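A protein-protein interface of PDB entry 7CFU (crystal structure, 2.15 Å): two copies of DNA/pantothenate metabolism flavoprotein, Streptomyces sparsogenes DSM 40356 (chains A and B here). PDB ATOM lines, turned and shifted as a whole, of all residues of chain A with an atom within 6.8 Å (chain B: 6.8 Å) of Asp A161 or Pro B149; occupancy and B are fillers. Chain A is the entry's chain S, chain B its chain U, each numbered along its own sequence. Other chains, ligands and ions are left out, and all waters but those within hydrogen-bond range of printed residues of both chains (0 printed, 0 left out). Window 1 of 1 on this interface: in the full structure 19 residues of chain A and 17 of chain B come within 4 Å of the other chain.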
ATOM      1  N   ALA A 115      26.691   1.206 -23.770  1.00  0.00           N
ATOM      2  CA  ALA A 115      25.661   0.241 -23.387  1.00  0.00           C
ATOM      3  C   ALA A 115      26.087  -0.577 -22.175  1.00  0.00           C
ATOM      4  O   ALA A 115      25.272  -0.856 -21.287  1.00  0.00           O
ATOM      5  CB  ALA A 115      25.341  -0.674 -24.569  1.00  0.00           C
ATOM      6  N   ALA A 116      27.366  -0.958 -22.112  1.00  0.00           N
ATOM      7  CA  ALA A 116      27.853  -1.767 -20.996  1.00  0.00           C
ATOM      8  C   ALA A 116      27.821  -1.003 -19.677  1.00  0.00           C
ATOM      9  O   ALA A 116      27.728  -1.621 -18.611  1.00  0.00           O
ATOM     10  CB  ALA A 116      29.272  -2.267 -21.274  1.00  0.00           C
ATOM     11  N   HIS A 117      27.906   0.325 -19.716  1.00  0.00           N
ATOM     12  CA  HIS A 117      28.015   1.113 -18.494  1.00  0.00           C
ATOM     13  C   HIS A 117      26.777   1.942 -18.191  1.00  0.00           C
ATOM     14  O   HIS A 117      26.802   2.752 -17.259  1.00  0.00           O
ATOM     15  CB  HIS A 117      29.247   2.011 -18.573  1.00  0.00           C
ATOM     16  CG  HIS A 117      30.529   1.246 -18.650  1.00  0.00           C
ATOM     17  ND1 HIS A 117      31.149   0.947 -19.844  1.00  0.00           N
ATOM     18  CD2 HIS A 117      31.293   0.695 -17.679  1.00  0.00           C
ATOM     19  CE1 HIS A 117      32.249   0.254 -19.604  1.00  0.00           C
ATOM     20  NE2 HIS A 117      32.359   0.088 -18.298  1.00  0.00           N
ATOM     21  N   ASP A 156      31.896  -8.717 -22.916  1.00  0.00           N
ATOM     22  CA  ASP A 156      31.563  -9.679 -21.865  1.00  0.00           C
ATOM     23  C   ASP A 156      30.468  -9.139 -20.958  1.00  0.00           C
ATOM     24  O   ASP A 156      29.529  -9.860 -20.597  1.00  0.00           O
ATOM     25  CB  ASP A 156      32.800 -10.028 -21.029  1.00  0.00           C
ATOM     26  CG  ASP A 156      33.897 -10.691 -21.847  1.00  0.00           C
ATOM     27  OD1 ASP A 156      33.596 -11.235 -22.932  1.00  0.00           O
ATOM     28  OD2 ASP A 156      35.066 -10.664 -21.397  1.00  0.00           O
ATOM     29  N   GLN A 157      30.587  -7.874 -20.556  1.00  0.00           N
ATOM     30  CA  GLN A 157      29.587  -7.301 -19.664  1.00  0.00           C
ATOM     31  C   GLN A 157      28.207  -7.298 -20.312  1.00  0.00           C
ATOM     32  O   GLN A 157      27.197  -7.546 -19.642  1.00  0.00           O
ATOM     33  CB  GLN A 157      29.994  -5.888 -19.266  1.00  0.00           C
ATOM     34  CG  GLN A 157      29.002  -5.211 -18.366  1.00  0.00           C
ATOM     35  CD  GLN A 157      28.879  -5.912 -17.042  1.00  0.00           C
ATOM     36  OE1 GLN A 157      28.047  -6.803 -16.870  1.00  0.00           O
ATOM     37  NE2 GLN A 157      29.707  -5.515 -16.089  1.00  0.00           N
ATOM     38  N   LEU A 158      28.143  -7.016 -21.617  1.00  0.00           N
ATOM     39  CA  LEU A 158      26.854  -6.977 -22.302  1.00  0.00           C
ATOM     40  C   LEU A 158      26.233  -8.367 -22.379  1.00  0.00           C
ATOM     41  O   LEU A 158      25.010  -8.517 -22.269  1.00  0.00           O
ATOM     42  CB  LEU A 158      27.016  -6.368 -23.700  1.00  0.00           C
ATOM     43  CG  LEU A 158      27.223  -4.848 -23.744  1.00  0.00           C
ATOM     44  CD1 LEU A 158      27.771  -4.400 -25.091  1.00  0.00           C
ATOM     45  CD2 LEU A 158      25.908  -4.120 -23.421  1.00  0.00           C
ATOM     46  N   ARG A 159      27.065  -9.394 -22.588  1.00  0.00           N
ATOM     47  CA  ARG A 159      26.577 -10.769 -22.581  1.00  0.00           C
ATOM     48  C   ARG A 159      26.025 -11.159 -21.217  1.00  0.00           C
ATOM     49  O   ARG A 159      24.976 -11.809 -21.130  1.00  0.00           O
ATOM     50  CB  ARG A 159      27.686 -11.717 -23.021  1.00  0.00           C
ATOM     51  CG  ARG A 159      27.902 -11.681 -24.517  1.00  0.00           C
ATOM     52  CD  ARG A 159      29.069 -12.539 -24.957  1.00  0.00           C
ATOM     53  NE  ARG A 159      29.071 -12.698 -26.406  1.00  0.00           N
ATOM     54  CZ  ARG A 159      30.167 -12.775 -27.154  1.00  0.00           C
ATOM     55  NH1 ARG A 159      31.367 -12.699 -26.596  1.00  0.00           N
ATOM     56  NH2 ARG A 159      30.054 -12.922 -28.467  1.00  0.00           N
ATOM     57  N   GLU A 160      26.711 -10.773 -20.139  1.00  0.00           N
ATOM     58  CA  GLU A 160      26.195 -11.054 -18.803  1.00  0.00           C
ATOM     59  C   GLU A 160      24.868 -10.351 -18.547  1.00  0.00           C
ATOM     60  O   GLU A 160      24.014 -10.883 -17.827  1.00  0.00           O
ATOM     61  CB  GLU A 160      27.214 -10.639 -17.746  1.00  0.00           C
ATOM     62  CG  GLU A 160      28.507 -11.431 -17.800  1.00  0.00           C
ATOM     63  CD  GLU A 160      29.500 -10.986 -16.747  1.00  0.00           C
ATOM     64  OE1 GLU A 160      30.649 -11.481 -16.764  1.00  0.00           O
ATOM     65  OE2 GLU A 160      29.130 -10.136 -15.907  1.00  0.00           O
ATOM     66  N   ASP A 161      24.661  -9.183 -19.151  1.00  0.00           N
ATOM     67  CA  ASP A 161      23.423  -8.433 -18.982  1.00  0.00           C
ATOM     68  C   ASP A 161      22.288  -8.954 -19.857  1.00  0.00           C
ATOM     69  O   ASP A 161      21.178  -8.422 -19.775  1.00  0.00           O
ATOM     70  CB  ASP A 161      23.670  -6.952 -19.276  1.00  0.00           C
ATOM     71  CG  ASP A 161      24.538  -6.282 -18.223  1.00  0.00           C
ATOM     72  OD1 ASP A 161      24.752  -6.887 -17.147  1.00  0.00           O
ATOM     73  OD2 ASP A 161      25.029  -5.161 -18.484  1.00  0.00           O
ATOM     74  N   GLY A 162      22.531  -9.972 -20.677  1.00  0.00           N
ATOM     75  CA  GLY A 162      21.487 -10.583 -21.468  1.00  0.00           C
ATOM     76  C   GLY A 162      21.428 -10.193 -22.928  1.00  0.00           C
ATOM     77  O   GLY A 162      20.479 -10.592 -23.612  1.00  0.00           O
ATOM     78  N   TYR A 163      22.403  -9.440 -23.435  1.00  0.00           N
ATOM     79  CA  TYR A 163      22.386  -9.022 -24.831  1.00  0.00           C
ATOM     80  C   TYR A 163      23.043 -10.071 -25.726  1.00  0.00           C
ATOM     81  O   TYR A 163      24.036 -10.697 -25.350  1.00  0.00           O
ATOM     82  CB  TYR A 163      23.083  -7.665 -24.999  1.00  0.00           C
ATOM     83  CG  TYR A 163      22.336  -6.533 -24.321  1.00  0.00           C
ATOM     84  CD1 TYR A 163      21.248  -5.918 -24.943  1.00  0.00           C
ATOM     85  CD2 TYR A 163      22.716  -6.078 -23.069  1.00  0.00           C
ATOM     86  CE1 TYR A 163      20.546  -4.893 -24.317  1.00  0.00           C
ATOM     87  CE2 TYR A 163      22.029  -5.054 -22.438  1.00  0.00           C
ATOM     88  CZ  TYR A 163      20.943  -4.465 -23.067  1.00  0.00           C
ATOM     89  OH  TYR A 163      20.261  -3.449 -22.437  1.00  0.00           O
ATOM     90  N   MET B 145      13.931   1.527 -17.076  1.00  0.00           N
ATOM     91  CA  MET B 145      15.309   2.012 -16.979  1.00  0.00           C
ATOM     92  C   MET B 145      15.912   1.705 -15.615  1.00  0.00           C
ATOM     93  O   MET B 145      17.049   1.229 -15.524  1.00  0.00           O
ATOM     94  CB  MET B 145      15.358   3.515 -17.256  1.00  0.00           C
ATOM     95  CG  MET B 145      14.787   3.907 -18.624  1.00  0.00           C
ATOM     96  SD  MET B 145      14.454   5.680 -18.791  1.00  0.00           S
ATOM     97  CE  MET B 145      16.128   6.332 -18.736  1.00  0.00           C
ATOM     98  N   TRP B 146      15.155   1.946 -14.543  1.00  0.00           N
ATOM     99  CA  TRP B 146      15.668   1.708 -13.199  1.00  0.00           C
ATOM    100  C   TRP B 146      16.046   0.246 -12.977  1.00  0.00           C
ATOM    101  O   TRP B 146      16.965  -0.046 -12.203  1.00  0.00           O
ATOM    102  CB  TRP B 146      14.630   2.166 -12.179  1.00  0.00           C
ATOM    103  CG  TRP B 146      15.044   2.032 -10.760  1.00  0.00           C
ATOM    104  CD1 TRP B 146      14.516   1.184  -9.828  1.00  0.00           C
ATOM    105  CD2 TRP B 146      16.091   2.754 -10.104  1.00  0.00           C
ATOM    106  NE1 TRP B 146      15.162   1.349  -8.623  1.00  0.00           N
ATOM    107  CE2 TRP B 146      16.134   2.305  -8.767  1.00  0.00           C
ATOM    108  CE3 TRP B 146      16.993   3.742 -10.516  1.00  0.00           C
ATOM    109  CZ2 TRP B 146      17.045   2.806  -7.839  1.00  0.00           C
ATOM    110  CZ3 TRP B 146      17.898   4.244  -9.590  1.00  0.00           C
ATOM    111  CH2 TRP B 146      17.917   3.772  -8.266  1.00  0.00           C
ATOM    112  N   SER B 147      15.378  -0.679 -13.664  1.00  0.00           N
ATOM    113  CA  SER B 147      15.636  -2.098 -13.464  1.00  0.00           C
ATOM    114  C   SER B 147      16.821  -2.618 -14.273  1.00  0.00           C
ATOM    115  O   SER B 147      17.198  -3.781 -14.098  1.00  0.00           O
ATOM    116  CB  SER B 147      14.390  -2.912 -13.825  1.00  0.00           C
ATOM    117  OG  SER B 147      14.241  -2.982 -15.233  1.00  0.00           O
ATOM    118  N   LYS B 148      17.413  -1.811 -15.151  1.00  0.00           N
ATOM    119  CA  LYS B 148      18.517  -2.306 -15.965  1.00  0.00           C
ATOM    120  C   LYS B 148      19.718  -2.651 -15.086  1.00  0.00           C
ATOM    121  O   LYS B 148      20.029  -1.919 -14.140  1.00  0.00           O
ATOM    122  CB  LYS B 148      18.920  -1.282 -17.028  1.00  0.00           C
ATOM    123  CG  LYS B 148      17.990  -1.221 -18.234  1.00  0.00           C
ATOM    124  CD  LYS B 148      18.011  -2.544 -18.987  1.00  0.00           C
ATOM    125  CE  LYS B 148      17.340  -2.430 -20.347  1.00  0.00           C
ATOM    126  NZ  LYS B 148      15.938  -1.998 -20.224  1.00  0.00           N
ATOM    127  N   PRO B 149      20.403  -3.767 -15.359  1.00  0.00           N
ATOM    128  CA  PRO B 149      21.592  -4.121 -14.555  1.00  0.00           C
ATOM    129  C   PRO B 149      22.673  -3.048 -14.543  1.00  0.00           C
ATOM    130  O   PRO B 149      23.261  -2.787 -13.485  1.00  0.00           O
ATOM    131  CB  PRO B 149      22.100  -5.407 -15.229  1.00  0.00           C
ATOM    132  CG  PRO B 149      20.956  -5.943 -15.982  1.00  0.00           C
ATOM    133  CD  PRO B 149      20.111  -4.769 -16.394  1.00  0.00           C
ATOM    134  N   ALA B 150      22.954  -2.419 -15.689  1.00  0.00           N
ATOM    135  CA  ALA B 150      23.984  -1.382 -15.728  1.00  0.00           C
ATOM    136  C   ALA B 150      23.625  -0.217 -14.818  1.00  0.00           C
ATOM    137  O   ALA B 150      24.486   0.318 -14.111  1.00  0.00           O
ATOM    138  CB  ALA B 150      24.201  -0.897 -17.163  1.00  0.00           C
ATOM    139  N   VAL B 151      22.353   0.183 -14.815  1.00  0.00           N
ATOM    140  CA  VAL B 151      21.919   1.283 -13.958  1.00  0.00           C
ATOM    141  C   VAL B 151      22.114   0.916 -12.490  1.00  0.00           C
ATOM    142  O   VAL B 151      22.639   1.707 -11.699  1.00  0.00           O
ATOM    143  CB  VAL B 151      20.456   1.655 -14.263  1.00  0.00           C
ATOM    144  CG1 VAL B 151      19.945   2.726 -13.296  1.00  0.00           C
ATOM    145  CG2 VAL B 151      20.317   2.103 -15.702  1.00  0.00           C
ATOM    146  N   GLN B 152      21.721  -0.304 -12.108  1.00  0.00           N
ATOM    147  CA  GLN B 152      21.847  -0.681 -10.701  1.00  0.00           C
ATOM    148  C   GLN B 152      23.305  -0.838 -10.297  1.00  0.00           C
ATOM    149  O   GLN B 152      23.657  -0.561  -9.147  1.00  0.00           O
ATOM    150  CB  GLN B 152      21.054  -1.956 -10.406  1.00  0.00           C
ATOM    151  CG  GLN B 152      19.541  -1.718 -10.379  1.00  0.00           C
ATOM    152  CD  GLN B 152      19.152  -0.509  -9.522  1.00  0.00           C
ATOM    153  OE1 GLN B 152      19.577  -0.384  -8.367  1.00  0.00           O
ATOM    154  NE2 GLN B 152      18.366   0.401 -10.100  1.00  0.00           N
ATOM    155  N   ARG B 153      24.166  -1.275 -11.222  1.00  0.00           N
ATOM    156  CA  ARG B 153      25.598  -1.258 -10.942  1.00  0.00           C
ATOM    157  C   ARG B 153      26.077   0.149 -10.619  1.00  0.00           C
ATOM    158  O   ARG B 153      26.884   0.340  -9.703  1.00  0.00           O
ATOM    159  CB  ARG B 153      26.384  -1.826 -12.123  1.00  0.00           C
ATOM    160  CG  ARG B 153      26.340  -3.325 -12.218  1.00  0.00           C
ATOM    161  CD  ARG B 153      27.423  -3.850 -13.142  1.00  0.00           C
ATOM    162  NE  ARG B 153      27.230  -3.451 -14.535  1.00  0.00           N
ATOM    163  CZ  ARG B 153      26.453  -4.101 -15.394  1.00  0.00           C
ATOM    164  NH1 ARG B 153      25.786  -5.175 -14.998  1.00  0.00           N
ATOM    165  NH2 ARG B 153      26.344  -3.682 -16.648  1.00  0.00           N
ATOM    166  N   ASN B 154      25.575   1.148 -11.353  1.00  0.00           N
ATOM    167  CA  ASN B 154      25.984   2.527 -11.121  1.00  0.00           C
ATOM    168  C   ASN B 154      25.471   3.036  -9.780  1.00  0.00           C
ATOM    169  O   ASN B 154      26.195   3.735  -9.062  1.00  0.00           O
ATOM    170  CB  ASN B 154      25.505   3.413 -12.277  1.00  0.00           C
ATOM    171  CG  ASN B 154      26.146   3.022 -13.600  1.00  0.00           C
ATOM    172  OD1 ASN B 154      27.257   2.501 -13.621  1.00  0.00           O
ATOM    173  ND2 ASN B 154      25.457   3.274 -14.704  1.00  0.00           N
ATOM    174  N   ASP B 156      24.825   1.143  -7.106  1.00  0.00           N
ATOM    175  CA  ASP B 156      25.642   0.489  -6.083  1.00  0.00           C
ATOM    176  C   ASP B 156      27.027   1.116  -5.995  1.00  0.00           C
ATOM    177  O   ASP B 156      27.540   1.354  -4.895  1.00  0.00           O
ATOM    178  CB  ASP B 156      25.765  -1.013  -6.356  1.00  0.00           C
ATOM    179  CG  ASP B 156      24.435  -1.736  -6.267  1.00  0.00           C
ATOM    180  OD1 ASP B 156      23.502  -1.199  -5.631  1.00  0.00           O
ATOM    181  OD2 ASP B 156      24.328  -2.850  -6.826  1.00  0.00           O
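The guanidinium group (NH2) of Arg B153 lies within hydrogen-bond range of the backbone carbonyl oxygen (O) of Ala A116 (3.2 Å).
The side-chain amide nitrogen (ND2) of Asn B154 is in hydrogen-bond range of the backbone carbonyl oxygen (O) of His A117.
The guanidinium group (NH1) of Arg B153 is in hydrogen-bond range of the side-chain amide oxygen (OE1) of Gln A157 (3.4 Å).
NH2 of Arg B153 lies within salt-bridge range of OD2 of Asp A161 (2.7 Å).
Of the 11 printed residues of chain B, 5 touch a printed residue of chain A.
Printed residues of chain B that touch a printed residue of chain A: Lys B148, Pro B149, Ala B150, Arg B153 and Asn B154.
Printed residues of chain A that touch a printed residue of chain B: Ala A116, His A117, Gln A157, Asp A161 and Tyr A163.
Hydrophobic or aromatic side chains of chain A that line the printed part of chain B: Tyr A163.
Position printed for both chains: 156.
OE1 of Gln A157 sits close to OD1 of Asp A161 (3.3 Å).
The backbone carbonyl oxygen (O) of Leu A158 is in hydrogen-bond range of the backbone NH (N) of Tyr A163.
The backbone carbonyl oxygen of Ala B150 lies within hydrogen-bond range of the side-chain amide nitrogen of Asn B154, 3.2 Å away.
Of chain B, only Pro B149 (3.6 Å) and Arg B153 (2.7 Å) come within 4 Å of Asp A161.
Of chain A, only Asp A161 comes within 4 Å of Pro B149.
Of the printed residues of chain A, Arg B153 touches Ala A116 (3.2 Å), Gln A157 (3.4 Å) and Asp A161 (2.7 Å).
Printed residues of chain A within 4 Å of Ala B150: Ala A116 (3.9 Å) and His A117 (3.97 Å).
Of the printed residues of chain B, His A117 touches Ala B150 and Asn B154.
Of the printed residues of chain A, Asn B154 touches His A117 (2.9 Å).
Gly A162 touches none of the printed residues of chain B.
Trp B146 touches none of the printed residues of chain A.
The nearest printed residue of chain A that does not touch Arg B153 is His A117 (5.3 Å).
Among the printed residues, pairs that only touch across the chains: Asp A161 with Pro B149, Tyr A163 with Lys B148, Ala A116 with Ala B150 and His A117 with Ala B150.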
